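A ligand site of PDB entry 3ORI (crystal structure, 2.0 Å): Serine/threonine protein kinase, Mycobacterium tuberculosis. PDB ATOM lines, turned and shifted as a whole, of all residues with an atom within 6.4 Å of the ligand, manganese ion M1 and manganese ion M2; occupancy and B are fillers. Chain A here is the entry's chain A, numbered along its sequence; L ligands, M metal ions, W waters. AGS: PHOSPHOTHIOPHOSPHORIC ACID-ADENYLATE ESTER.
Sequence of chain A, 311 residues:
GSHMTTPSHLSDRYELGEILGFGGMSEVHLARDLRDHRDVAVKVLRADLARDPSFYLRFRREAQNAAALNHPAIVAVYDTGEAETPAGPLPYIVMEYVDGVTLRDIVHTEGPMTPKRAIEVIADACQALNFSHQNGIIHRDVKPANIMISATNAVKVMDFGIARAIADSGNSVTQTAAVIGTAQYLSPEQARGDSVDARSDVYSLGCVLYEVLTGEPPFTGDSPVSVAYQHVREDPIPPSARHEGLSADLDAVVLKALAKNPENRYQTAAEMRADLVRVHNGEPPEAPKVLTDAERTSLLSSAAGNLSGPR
Water W3 bridges OE2 of Glu 62 and NH2 of Arg 58.
Water W8 lies within hydrogen-bond range of O2' of the ligand (2.4 Å) and OD2 of Asp 105 (3.2 Å).
Water W6 lies within hydrogen-bond range of the backbone carbonyl oxygen of Ala 145 (2.6 Å) and an oxygen (O3') of the ligand (2.8 Å).
Water W1 bridges O1A of the ligand (3.0 Å) and SD of Met 95 (3.4 Å).
Water W5 bridges OD2 of Asp 141 (2.8 Å) and S1G of the ligand (3.3 Å).
Water W7 lies within hydrogen-bond range of OG1 of Thr 102 (2.8 Å), OD1 of Asp 105 (2.9 Å), NH2 of Arg 104 (3.0 Å) and O3' of the ligand (3.4 Å).
The side-chain amino group of Lys 43 lies close to the side-chain carboxylate of Asp 159.
O of Asn 146 sits at hydrogen-bond distance from N of Met 158 (3.0 Å).
The backbone carbonyl oxygen (O) of Ala 76 lies within hydrogen-bond range of the backbone NH (N) of Glu 96, 2.9 Å away.
The guanidinium group (NE) of Arg 58 lies close to the side-chain sulfur (SD) of Met 25, 3.5 Å away.
N of Met 95 lies within hydrogen-bond range of O of Ala 41, at 2.8 Å.
N of Val 28 is in hydrogen-bond range of O of Gly 21, at 3.0 Å.
The side-chain hydroxyl (OG1) of Thr 102 sits close to the backbone NH (N) of Arg 104 (3.4 Å).
The side-chain hydroxyl of Thr 102 sits at hydrogen-bond distance from the backbone NH of Asp 105 (2.9 Å).
Manganese ion M2 is bound by O2A of the ligand (2.1 Å), OD2 of Asp 159 (2.4 Å), OD1 of Asn 146 (2.4 Å) and O3G of the ligand (2.5 Å).
Manganese ion M2 has four donor atoms within binding distance.
Slightly farther from manganese ion M2 lies an oxygen (O3B) of the ligand (2.8 Å).
SD of Met 158 sits close to N7 of the ligand (3.8 Å).
Residues that only touch the ligand: Leu 20, Gly 21, Phe 22, Gly 23, Val 28, Ala 41, Val 75, Tyr 97, Thr 102, Arg 104, Asp 141 and Met 148.
Along chain A the residues within 4 Å of the ligand span positions 20 to 159.
Of the 34 residues printed, 2 come within 4 Å of manganese ion M2.
The nearest printed residue that does not touch manganese ion M2 is Lys 143 (4.1 Å).
An oxygen (O1A) of the ligand is in salt-bridge range of the side-chain amino group (NZ) of Lys 43 (2.5 Å).
NZ of Lys 143 sits close to O3G of the ligand (2.5 Å).
A nitrogen (N6) of the ligand is in hydrogen-bond range of the backbone carbonyl oxygen of Glu 96 (2.7 Å).
An oxygen (O2G) of the ligand sits at hydrogen-bond distance from the backbone NH (N) of Gly 24.
The backbone NH (N) of Met 25 sits at hydrogen-bond distance from an oxygen (O1B) of the ligand (2.9 Å).
The backbone NH of Ser 26 sits at hydrogen-bond distance from an oxygen (O1B) of the ligand (3.4 Å).
An oxygen (O1B) of the ligand is in hydrogen-bond range of the side-chain hydroxyl of Ser 26 (3.0 Å).
The backbone NH (N) of Val 98 is in hydrogen-bond range of a nitrogen (N1) of the ligand (3.1 Å).
SD of Met 95 lies close to N6 of the ligand.
Lys 43 touches manganese ion M1.
Two residues have an atom within 4 Å of manganese ion M1: Lys 43 and Asp 159.
The nearest printed residue that does not touch manganese ion M1 is Glu 62 (4.01 Å).
Water W4 binds manganese ion M1, at 1.8 Å.
An oxygen (O2B) of the ligand binds manganese ion M1, at 2.2 Å.
Water W3 is bound to manganese ion M1.
The side-chain carboxylate (OD2) of Asp 159 is bound to manganese ion M1, 2.3 Å away.
The side-chain carboxylate (OD1) of Asp 159 binds manganese ion M1, at 2.3 Å.
Manganese ion M1 has five donor atoms within binding distance.
Slightly farther from manganese ion M1 lies a sulfur (S1G) of the ligand (2.9 Å).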
ATOM      1  N   LEU A  20      16.039  33.648  19.738  1.00  0.00           N
ATOM      2  CA  LEU A  20      16.512  32.436  19.041  1.00  0.00           C
ATOM      3  C   LEU A  20      15.971  32.400  17.633  1.00  0.00           C
ATOM      4  O   LEU A  20      16.623  31.895  16.711  1.00  0.00           O
ATOM      5  CB  LEU A  20      16.045  31.200  19.777  1.00  0.00           C
ATOM      6  CG  LEU A  20      16.805  30.935  21.071  1.00  0.00           C
ATOM      7  CD1 LEU A  20      16.131  29.881  21.941  1.00  0.00           C
ATOM      8  CD2 LEU A  20      18.233  30.523  20.732  1.00  0.00           C
ATOM      9  N   GLY A  21      14.754  32.924  17.479  1.00  0.00           N
ATOM     10  CA  GLY A  21      14.106  32.933  16.196  1.00  0.00           C
ATOM     11  C   GLY A  21      12.827  33.721  16.164  1.00  0.00           C
ATOM     12  O   GLY A  21      12.242  34.059  17.181  1.00  0.00           O
ATOM     13  N   PHE A  22      12.391  33.995  14.950  1.00  0.00           N
ATOM     14  CA  PHE A  22      11.137  34.664  14.695  1.00  0.00           C
ATOM     15  C   PHE A  22      10.252  33.755  13.859  1.00  0.00           C
ATOM     16  O   PHE A  22      10.718  33.214  12.855  1.00  0.00           O
ATOM     17  CB  PHE A  22      11.392  35.958  13.913  1.00  0.00           C
ATOM     18  CG  PHE A  22      12.161  36.999  14.674  1.00  0.00           C
ATOM     19  CD1 PHE A  22      13.515  37.163  14.466  1.00  0.00           C
ATOM     20  CD2 PHE A  22      11.528  37.814  15.595  1.00  0.00           C
ATOM     21  CE1 PHE A  22      14.224  38.132  15.161  1.00  0.00           C
ATOM     22  CE2 PHE A  22      12.224  38.783  16.288  1.00  0.00           C
ATOM     23  CZ  PHE A  22      13.572  38.947  16.071  1.00  0.00           C
ATOM     24  N   GLY A  23       8.998  33.600  14.265  1.00  0.00           N
ATOM     25  CA  GLY A  23       7.992  33.027  13.409  1.00  0.00           C
ATOM     26  C   GLY A  23       6.914  34.053  13.075  1.00  0.00           C
ATOM     27  O   GLY A  23       6.962  35.208  13.518  1.00  0.00           O
ATOM     28  N   GLY A  24       5.936  33.595  12.303  1.00  0.00           N
ATOM     29  CA  GLY A  24       4.811  34.420  11.926  1.00  0.00           C
ATOM     30  C   GLY A  24       3.931  34.931  13.050  1.00  0.00           C
ATOM     31  O   GLY A  24       3.286  35.950  12.917  1.00  0.00           O
ATOM     32  N   MET A  25       3.902  34.243  14.172  1.00  0.00           N
ATOM     33  CA  MET A  25       3.031  34.632  15.273  1.00  0.00           C
ATOM     34  C   MET A  25       3.771  35.011  16.565  1.00  0.00           C
ATOM     35  O   MET A  25       3.140  35.408  17.537  1.00  0.00           O
ATOM     36  CB  MET A  25       2.109  33.450  15.595  1.00  0.00           C
ATOM     37  CG  MET A  25       0.796  33.434  14.861  1.00  0.00           C
ATOM     38  SD  MET A  25      -0.103  31.924  15.254  1.00  0.00           S
ATOM     39  CE  MET A  25      -0.336  32.029  17.040  1.00  0.00           C
ATOM     40  N   SER A  26       5.098  34.893  16.585  1.00  0.00           N
ATOM     41  CA  SER A  26       5.817  34.899  17.847  1.00  0.00           C
ATOM     42  C   SER A  26       7.284  35.212  17.702  1.00  0.00           C
ATOM     43  O   SER A  26       7.863  35.091  16.621  1.00  0.00           O
ATOM     44  CB  SER A  26       5.721  33.536  18.496  1.00  0.00           C
ATOM     45  OG  SER A  26       6.462  32.588  17.749  1.00  0.00           O
ATOM     46  N   GLU A  27       7.861  35.627  18.823  1.00  0.00           N
ATOM     47  CA  GLU A  27       9.291  35.718  19.031  1.00  0.00           C
ATOM     48  C   GLU A  27       9.666  34.659  20.044  1.00  0.00           C
ATOM     49  O   GLU A  27       9.012  34.541  21.100  1.00  0.00           O
ATOM     50  CB  GLU A  27       9.667  37.052  19.685  1.00  0.00           C
ATOM     51  CG  GLU A  27       9.258  38.263  18.934  1.00  0.00           C
ATOM     52  CD  GLU A  27       9.879  39.547  19.495  1.00  0.00           C
ATOM     53  OE1 GLU A  27      10.367  39.538  20.655  1.00  0.00           O
ATOM     54  OE2 GLU A  27       9.830  40.570  18.762  1.00  0.00           O
ATOM     55  N   VAL A  28      10.706  33.898  19.728  1.00  0.00           N
ATOM     56  CA  VAL A  28      11.210  32.894  20.635  1.00  0.00           C
ATOM     57  C   VAL A  28      12.554  33.350  21.236  1.00  0.00           C
ATOM     58  O   VAL A  28      13.541  33.536  20.512  1.00  0.00           O
ATOM     59  CB  VAL A  28      11.340  31.513  19.984  1.00  0.00           C
ATOM     60  CG1 VAL A  28      11.830  30.479  21.007  1.00  0.00           C
ATOM     61  CG2 VAL A  28       9.978  31.059  19.394  1.00  0.00           C
ATOM     62  N   ALA A  41      13.417  27.673  26.107  1.00  0.00           N
ATOM     63  CA  ALA A  41      13.012  28.559  25.036  1.00  0.00           C
ATOM     64  C   ALA A  41      11.659  29.110  25.416  1.00  0.00           C
ATOM     65  O   ALA A  41      10.785  28.363  25.821  1.00  0.00           O
ATOM     66  CB  ALA A  41      12.964  27.807  23.679  1.00  0.00           C
ATOM     67  N   LYS A  43       8.473  31.137  23.957  1.00  0.00           N
ATOM     68  CA  LYS A  43       7.757  31.620  22.792  1.00  0.00           C
ATOM     69  C   LYS A  43       6.752  32.633  23.276  1.00  0.00           C
ATOM     70  O   LYS A  43       5.917  32.328  24.110  1.00  0.00           O
ATOM     71  CB  LYS A  43       7.053  30.444  22.137  1.00  0.00           C
ATOM     72  CG  LYS A  43       6.270  30.713  20.881  1.00  0.00           C
ATOM     73  CD  LYS A  43       6.025  29.369  20.192  1.00  0.00           C
ATOM     74  CE  LYS A  43       5.068  29.443  19.029  1.00  0.00           C
ATOM     75  NZ  LYS A  43       5.144  28.186  18.253  1.00  0.00           N
ATOM     76  N   ARG A  58      -5.708  30.963  19.143  1.00  0.00           N
ATOM     77  CA  ARG A  58      -4.860  30.002  18.436  1.00  0.00           C
ATOM     78  C   ARG A  58      -3.589  29.673  19.234  1.00  0.00           C
ATOM     79  O   ARG A  58      -3.237  28.493  19.416  1.00  0.00           O
ATOM     80  CB  ARG A  58      -4.457  30.530  17.049  1.00  0.00           C
ATOM     81  CG  ARG A  58      -3.533  29.610  16.268  1.00  0.00           C
ATOM     82  CD  ARG A  58      -3.280  30.115  14.870  1.00  0.00           C
ATOM     83  NE  ARG A  58      -2.240  29.330  14.236  1.00  0.00           N
ATOM     84  CZ  ARG A  58      -1.638  29.644  13.087  1.00  0.00           C
ATOM     85  NH1 ARG A  58      -1.976  30.745  12.391  1.00  0.00           N
ATOM     86  NH2 ARG A  58      -0.673  28.836  12.619  1.00  0.00           N
ATOM     87  N   GLU A  62      -2.606  25.897  20.722  1.00  0.00           N
ATOM     88  CA  GLU A  62      -1.399  25.226  20.261  1.00  0.00           C
ATOM     89  C   GLU A  62      -0.552  24.736  21.428  1.00  0.00           C
ATOM     90  O   GLU A  62      -0.037  23.632  21.385  1.00  0.00           O
ATOM     91  CB  GLU A  62      -0.597  26.170  19.350  1.00  0.00           C
ATOM     92  CG  GLU A  62      -1.226  26.259  17.934  1.00  0.00           C
ATOM     93  CD  GLU A  62      -0.530  27.228  17.018  1.00  0.00           C
ATOM     94  OE1 GLU A  62       0.247  28.058  17.523  1.00  0.00           O
ATOM     95  OE2 GLU A  62      -0.797  27.192  15.804  1.00  0.00           O
ATOM     96  N   VAL A  75       9.618  18.554  20.576  1.00  0.00           N
ATOM     97  CA  VAL A  75       9.949  19.613  21.541  1.00  0.00           C
ATOM     98  C   VAL A  75       8.921  19.732  22.680  1.00  0.00           C
ATOM     99  O   VAL A  75       7.726  20.017  22.428  1.00  0.00           O
ATOM    100  CB  VAL A  75      10.054  20.939  20.817  1.00  0.00           C
ATOM    101  CG1 VAL A  75      10.082  22.115  21.792  1.00  0.00           C
ATOM    102  CG2 VAL A  75      11.316  20.902  19.870  1.00  0.00           C
ATOM    103  N   ALA A  76       9.393  19.497  23.907  1.00  0.00           N
ATOM    104  CA  ALA A  76       8.511  19.469  25.055  1.00  0.00           C
ATOM    105  C   ALA A  76       8.055  20.886  25.425  1.00  0.00           C
ATOM    106  O   ALA A  76       8.797  21.876  25.225  1.00  0.00           O
ATOM    107  CB  ALA A  76       9.191  18.779  26.252  1.00  0.00           C
ATOM    108  N   MET A  95       9.340  26.167  26.869  1.00  0.00           N
ATOM    109  CA  MET A  95       9.559  24.890  26.192  1.00  0.00           C
ATOM    110  C   MET A  95      10.999  24.513  26.188  1.00  0.00           C
ATOM    111  O   MET A  95      11.862  25.307  26.534  1.00  0.00           O
ATOM    112  CB  MET A  95       9.006  24.923  24.754  1.00  0.00           C
ATOM    113  CG  MET A  95       9.582  25.923  23.888  1.00  0.00           C
ATOM    114  SD  MET A  95       8.849  26.069  22.239  1.00  0.00           S
ATOM    115  CE  MET A  95       9.707  27.600  21.836  1.00  0.00           C
ATOM    116  N   GLU A  96      11.220  23.267  25.793  1.00  0.00           N
ATOM    117  CA  GLU A  96      12.513  22.706  25.640  1.00  0.00           C
ATOM    118  C   GLU A  96      13.356  23.542  24.661  1.00  0.00           C
ATOM    119  O   GLU A  96      12.927  23.802  23.536  1.00  0.00           O
ATOM    120  CB  GLU A  96      12.345  21.282  25.143  1.00  0.00           C
ATOM    121  CG  GLU A  96      13.567  20.456  25.034  1.00  0.00           C
ATOM    122  CD  GLU A  96      13.348  19.173  24.243  1.00  0.00           C
ATOM    123  OE1 GLU A  96      14.360  18.643  23.770  1.00  0.00           O
ATOM    124  OE2 GLU A  96      12.194  18.682  24.104  1.00  0.00           O
ATOM    125  N   TYR A  97      14.545  23.965  25.112  1.00  0.00           N
ATOM    126  CA  TYR A  97      15.558  24.600  24.247  1.00  0.00           C
ATOM    127  C   TYR A  97      16.257  23.563  23.353  1.00  0.00           C
ATOM    128  O   TYR A  97      16.731  22.538  23.818  1.00  0.00           O
ATOM    129  CB  TYR A  97      16.558  25.364  25.099  1.00  0.00           C
ATOM    130  CG  TYR A  97      17.791  25.879  24.396  1.00  0.00           C
ATOM    131  CD1 TYR A  97      17.688  26.653  23.258  1.00  0.00           C
ATOM    132  CD2 TYR A  97      19.063  25.630  24.917  1.00  0.00           C
ATOM    133  CE1 TYR A  97      18.798  27.129  22.610  1.00  0.00           C
ATOM    134  CE2 TYR A  97      20.207  26.125  24.283  1.00  0.00           C
ATOM    135  CZ  TYR A  97      20.065  26.870  23.124  1.00  0.00           C
ATOM    136  OH  TYR A  97      21.151  27.355  22.455  1.00  0.00           O
ATOM    137  N   VAL A  98      16.252  23.798  22.058  1.00  0.00           N
ATOM    138  CA  VAL A  98      17.013  23.023  21.090  1.00  0.00           C
ATOM    139  C   VAL A  98      18.149  23.965  20.655  1.00  0.00           C
ATOM    140  O   VAL A  98      17.903  24.992  19.986  1.00  0.00           O
ATOM    141  CB  VAL A  98      16.130  22.569  19.903  1.00  0.00           C
ATOM    142  CG1 VAL A  98      16.904  21.779  18.880  1.00  0.00           C
ATOM    143  CG2 VAL A  98      14.934  21.725  20.395  1.00  0.00           C
ATOM    144  N   ASP A  99      19.372  23.632  21.093  1.00  0.00           N
ATOM    145  CA  ASP A  99      20.570  24.295  20.594  1.00  0.00           C
ATOM    146  C   ASP A  99      20.870  23.665  19.225  1.00  0.00           C
ATOM    147  O   ASP A  99      21.420  22.554  19.126  1.00  0.00           O
ATOM    148  CB  ASP A  99      21.737  24.073  21.548  1.00  0.00           C
ATOM    149  CG  ASP A  99      22.990  24.841  21.140  1.00  0.00           C
ATOM    150  OD1 ASP A  99      23.062  25.374  19.997  1.00  0.00           O
ATOM    151  OD2 ASP A  99      23.898  24.887  21.997  1.00  0.00           O
ATOM    152  N   GLY A 100      20.504  24.390  18.184  1.00  0.00           N
ATOM    153  CA  GLY A 100      20.524  23.847  16.846  1.00  0.00           C
ATOM    154  C   GLY A 100      19.929  24.786  15.822  1.00  0.00           C
ATOM    155  O   GLY A 100      19.893  25.997  16.007  1.00  0.00           O
ATOM    156  N   THR A 102      17.040  24.877  12.174  1.00  0.00           N
ATOM    157  CA  THR A 102      15.917  24.243  11.501  1.00  0.00           C
ATOM    158  C   THR A 102      16.420  23.697  10.178  1.00  0.00           C
ATOM    159  O   THR A 102      17.503  24.075   9.693  1.00  0.00           O
ATOM    160  CB  THR A 102      14.762  25.209  11.242  1.00  0.00           C
ATOM    161  OG1 THR A 102      15.178  26.179  10.278  1.00  0.00           O
ATOM    162  CG2 THR A 102      14.335  25.931  12.545  1.00  0.00           C
ATOM    163  N   ARG A 104      14.966  24.391   7.423  1.00  0.00           N
ATOM    164  CA  ARG A 104      14.920  25.608   6.608  1.00  0.00           C
ATOM    165  C   ARG A 104      16.302  26.301   6.644  1.00  0.00           C
ATOM    166  O   ARG A 104      16.919  26.533   5.607  1.00  0.00           O
ATOM    167  CB  ARG A 104      13.834  26.593   7.062  1.00  0.00           C
ATOM    168  CG  ARG A 104      13.930  27.948   6.319  1.00  0.00           C
ATOM    169  CD  ARG A 104      12.813  28.883   6.618  1.00  0.00           C
ATOM    170  NE  ARG A 104      12.816  29.268   8.019  1.00  0.00           N
ATOM    171  CZ  ARG A 104      11.809  29.880   8.639  1.00  0.00           C
ATOM    172  NH1 ARG A 104      10.694  30.181   7.982  1.00  0.00           N
ATOM    173  NH2 ARG A 104      11.909  30.171   9.925  1.00  0.00           N
ATOM    174  N   ASP A 105      16.755  26.618   7.847  1.00  0.00           N
ATOM    175  CA  ASP A 105      18.080  27.204   8.017  1.00  0.00           C
ATOM    176  C   ASP A 105      19.174  26.346   7.387  1.00  0.00           C
ATOM    177  O   ASP A 105      20.042  26.892   6.700  1.00  0.00           O
ATOM    178  CB  ASP A 105      18.389  27.407   9.482  1.00  0.00           C
ATOM    179  CG  ASP A 105      17.517  28.467  10.153  1.00  0.00           C
ATOM    180  OD1 ASP A 105      16.954  29.358   9.453  1.00  0.00           O
ATOM    181  OD2 ASP A 105      17.419  28.355  11.413  1.00  0.00           O
ATOM    182  N   ASP A 141       1.082  21.024  10.098  1.00  0.00           N
ATOM    183  CA  ASP A 141       1.998  22.077   9.655  1.00  0.00           C
ATOM    184  C   ASP A 141       3.438  21.568   9.502  1.00  0.00           C
ATOM    185  O   ASP A 141       4.415  22.283   9.815  1.00  0.00           O
ATOM    186  CB  ASP A 141       1.947  23.249  10.656  1.00  0.00           C
ATOM    187  CG  ASP A 141       2.632  24.511  10.149  1.00  0.00           C
ATOM    188  OD1 ASP A 141       2.605  24.701   8.904  1.00  0.00           O
ATOM    189  OD2 ASP A 141       3.196  25.288  11.003  1.00  0.00           O
ATOM    190  N   LYS A 143       6.787  21.161   8.013  1.00  0.00           N
ATOM    191  CA  LYS A 143       7.508  22.028   7.097  1.00  0.00           C
ATOM    192  C   LYS A 143       8.942  22.182   7.607  1.00  0.00           C
ATOM    193  O   LYS A 143       9.217  21.922   8.768  1.00  0.00           O
ATOM    194  CB  LYS A 143       6.820  23.387   6.918  1.00  0.00           C
ATOM    195  CG  LYS A 143       6.750  24.245   8.145  1.00  0.00           C
ATOM    196  CD  LYS A 143       6.139  25.632   7.858  1.00  0.00           C
ATOM    197  CE  LYS A 143       5.960  26.421   9.168  1.00  0.00           C
ATOM    198  NZ  LYS A 143       5.530  27.867   8.988  1.00  0.00           N
ATOM    199  N   ALA A 145      10.863  24.533   8.582  1.00  0.00           N
ATOM    200  CA  ALA A 145      11.059  25.404   9.759  1.00  0.00           C
ATOM    201  C   ALA A 145      10.580  24.784  11.079  1.00  0.00           C
ATOM    202  O   ALA A 145      10.931  25.270  12.186  1.00  0.00           O
ATOM    203  CB  ALA A 145      10.383  26.747   9.525  1.00  0.00           C
ATOM    204  N   ASN A 146       9.758  23.746  10.989  1.00  0.00           N
ATOM    205  CA  ASN A 146       9.246  23.101  12.202  1.00  0.00           C
ATOM    206  C   ASN A 146       9.955  21.834  12.553  1.00  0.00           C
ATOM    207  O   ASN A 146       9.406  21.038  13.334  1.00  0.00           O
ATOM    208  CB  ASN A 146       7.766  22.816  12.058  1.00  0.00           C
ATOM    209  CG  ASN A 146       6.921  24.062  12.137  1.00  0.00           C
ATOM    210  OD1 ASN A 146       7.377  25.090  12.646  1.00  0.00           O
ATOM    211  ND2 ASN A 146       5.695  23.979  11.647  1.00  0.00           N
ATOM    212  N   MET A 148      13.913  20.875  13.789  1.00  0.00           N
ATOM    213  CA  MET A 148      15.267  21.259  14.115  1.00  0.00           C
ATOM    214  C   MET A 148      16.229  20.073  14.232  1.00  0.00           C
ATOM    215  O   MET A 148      15.809  18.927  14.461  1.00  0.00           O
ATOM    216  CB  MET A 148      15.284  22.019  15.421  1.00  0.00           C
ATOM    217  CG  MET A 148      14.609  23.379  15.281  1.00  0.00           C
ATOM    218  SD  MET A 148      14.597  24.450  16.699  1.00  0.00           S
ATOM    219  CE  MET A 148      16.281  24.997  16.750  1.00  0.00           C
ATOM    220  N   MET A 158       8.498  20.348  16.098  1.00  0.00           N
ATOM    221  CA  MET A 158       7.803  21.282  16.958  1.00  0.00           C
ATOM    222  C   MET A 158       6.656  21.995  16.280  1.00  0.00           C
ATOM    223  O   MET A 158       6.379  21.782  15.115  1.00  0.00           O
ATOM    224  CB  MET A 158       8.790  22.312  17.465  1.00  0.00           C
ATOM    225  CG  MET A 158       9.342  23.247  16.381  1.00  0.00           C
ATOM    226  SD  MET A 158      10.913  23.904  16.878  1.00  0.00           S
ATOM    227  CE  MET A 158      11.811  22.325  16.803  1.00  0.00           C
ATOM    228  N   ASP A 159       5.984  22.831  17.059  1.00  0.00           N
ATOM    229  CA  ASP A 159       4.911  23.706  16.587  1.00  0.00           C
ATOM    230  C   ASP A 159       3.806  22.902  15.932  1.00  0.00           C
ATOM    231  O   ASP A 159       3.378  23.195  14.842  1.00  0.00           O
ATOM    232  CB  ASP A 159       5.501  24.792  15.673  1.00  0.00           C
ATOM    233  CG  ASP A 159       4.516  25.966  15.370  1.00  0.00           C
ATOM    234  OD1 ASP A 159       3.688  26.382  16.194  1.00  0.00           O
ATOM    235  OD2 ASP A 159       4.598  26.490  14.244  1.00  0.00           O
ATOM    236  N   PHE A 160       3.364  21.862  16.620  1.00  0.00           N
ATOM    237  CA  PHE A 160       2.225  21.066  16.176  1.00  0.00           C
ATOM    238  C   PHE A 160       0.991  21.976  16.064  1.00  0.00           C
ATOM    239  O   PHE A 160       0.779  22.832  16.895  1.00  0.00           O
ATOM    240  CB  PHE A 160       1.954  19.938  17.151  1.00  0.00           C
ATOM    241  CG  PHE A 160       2.798  18.691  16.919  1.00  0.00           C
ATOM    242  CD1 PHE A 160       2.214  17.521  16.436  1.00  0.00           C
ATOM    243  CD2 PHE A 160       4.163  18.698  17.170  1.00  0.00           C
ATOM    244  CE1 PHE A 160       2.996  16.368  16.204  1.00  0.00           C
ATOM    245  CE2 PHE A 160       4.955  17.558  16.990  1.00  0.00           C
ATOM    246  CZ  PHE A 160       4.375  16.387  16.494  1.00  0.00           C
ATOM    247  N   GLY A 181       1.410  30.902   8.809  1.00  0.00           N
ATOM    248  CA  GLY A 181       2.660  30.653   8.103  1.00  0.00           C
ATOM    249  C   GLY A 181       2.450  30.285   6.654  1.00  0.00           C
ATOM    250  O   GLY A 181       1.349  30.442   6.099  1.00  0.00           O
ATOM    251  N   THR A 182       3.523  29.810   6.021  1.00  0.00           N
ATOM    252  CA  THR A 182       3.463  29.396   4.610  1.00  0.00           C
ATOM    253  C   THR A 182       2.523  28.193   4.377  1.00  0.00           C
ATOM    254  O   THR A 182       2.256  27.412   5.286  1.00  0.00           O
ATOM    255  CB  THR A 182       4.865  29.098   4.023  1.00  0.00           C
ATOM    256  OG1 THR A 182       4.740  28.779   2.625  1.00  0.00           O
ATOM    257  CG2 THR A 182       5.531  27.961   4.738  1.00  0.00           C
HETATM  258  PG  AGS L   1       5.061  29.911  12.096  1.00  0.00           P
HETATM  259  S1G AGS L   1       3.446  30.000  12.566  1.00  0.00           S
HETATM  260  O2G AGS L   1       5.261  31.126  11.163  1.00  0.00           O
HETATM  261  O3G AGS L   1       5.382  28.585  11.381  1.00  0.00           O
HETATM  262  PB  AGS L   1       5.664  30.390  14.913  1.00  0.00           P
HETATM  263  O1B AGS L   1       5.281  31.820  15.095  1.00  0.00           O
HETATM  264  O2B AGS L   1       4.708  29.514  15.682  1.00  0.00           O
HETATM  265  O3B AGS L   1       5.988  30.038  13.387  1.00  0.00           O
HETATM  266  PA  AGS L   1       7.915  28.822  15.807  1.00  0.00           P
HETATM  267  O1A AGS L   1       7.270  28.191  16.996  1.00  0.00           O
HETATM  268  O2A AGS L   1       7.830  27.807  14.661  1.00  0.00           O
HETATM  269  O3A AGS L   1       7.162  30.240  15.572  1.00  0.00           O
HETATM  270  O5' AGS L   1       9.431  29.240  16.159  1.00  0.00           O
HETATM  271  C5' AGS L   1      10.060  30.349  15.588  1.00  0.00           C
HETATM  272  C4' AGS L   1      11.573  30.113  15.508  1.00  0.00           C
HETATM  273  O4' AGS L   1      12.109  30.053  16.828  1.00  0.00           O
HETATM  274  C3' AGS L   1      12.054  28.840  14.796  1.00  0.00           C
HETATM  275  O3' AGS L   1      12.366  29.003  13.434  1.00  0.00           O
HETATM  276  C2' AGS L   1      13.342  28.563  15.498  1.00  0.00           C
HETATM  277  O2' AGS L   1      14.355  29.327  14.876  1.00  0.00           O
HETATM  278  C1' AGS L   1      13.158  29.129  16.892  1.00  0.00           C
HETATM  279  N9  AGS L   1      12.702  28.151  17.870  1.00  0.00           N
HETATM  280  C8  AGS L   1      11.391  27.784  18.084  1.00  0.00           C
HETATM  281  N7  AGS L   1      11.386  26.917  19.104  1.00  0.00           N
HETATM  282  C5  AGS L   1      12.648  26.731  19.523  1.00  0.00           C
HETATM  283  C6  AGS L   1      13.188  25.954  20.528  1.00  0.00           C
HETATM  284  N6  AGS L   1      12.379  25.242  21.315  1.00  0.00           N
HETATM  285  N1  AGS L   1      14.542  25.989  20.738  1.00  0.00           N
HETATM  286  C2  AGS L   1      15.387  26.750  19.961  1.00  0.00           C
HETATM  287  N3  AGS L   1      14.838  27.518  18.963  1.00  0.00           N
HETATM  288  C4  AGS L   1      13.491  27.513  18.759  1.00  0.00           C
HETATM  289 MN    MN M   1       3.211  28.193  14.823  1.00  0.00          MN
HETATM  290 MN    MN M   2       6.519  27.312  13.154  1.00  0.00          MN
HETATM  291  O   HOH W   1       8.337  26.148  18.893  1.00  0.00           O
HETATM  292  O   HOH W   2      16.772  28.545  17.406  1.00  0.00           O
HETATM  293  O   HOH W   3       1.224  27.447  14.320  1.00  0.00           O
HETATM  294  O   HOH W   4       2.489  28.583  16.444  1.00  0.00           O
HETATM  295  O   HOH W   5       2.176  27.870  10.439  1.00  0.00           O
HETATM  296  O   HOH W   6      10.013  27.630  12.880  1.00  0.00           O
HETATM  297  O   HOH W   7      14.455  28.847  10.800  1.00  0.00           O
HETATM  298  O   HOH W   8      16.619  28.591  14.544  1.00  0.00           O
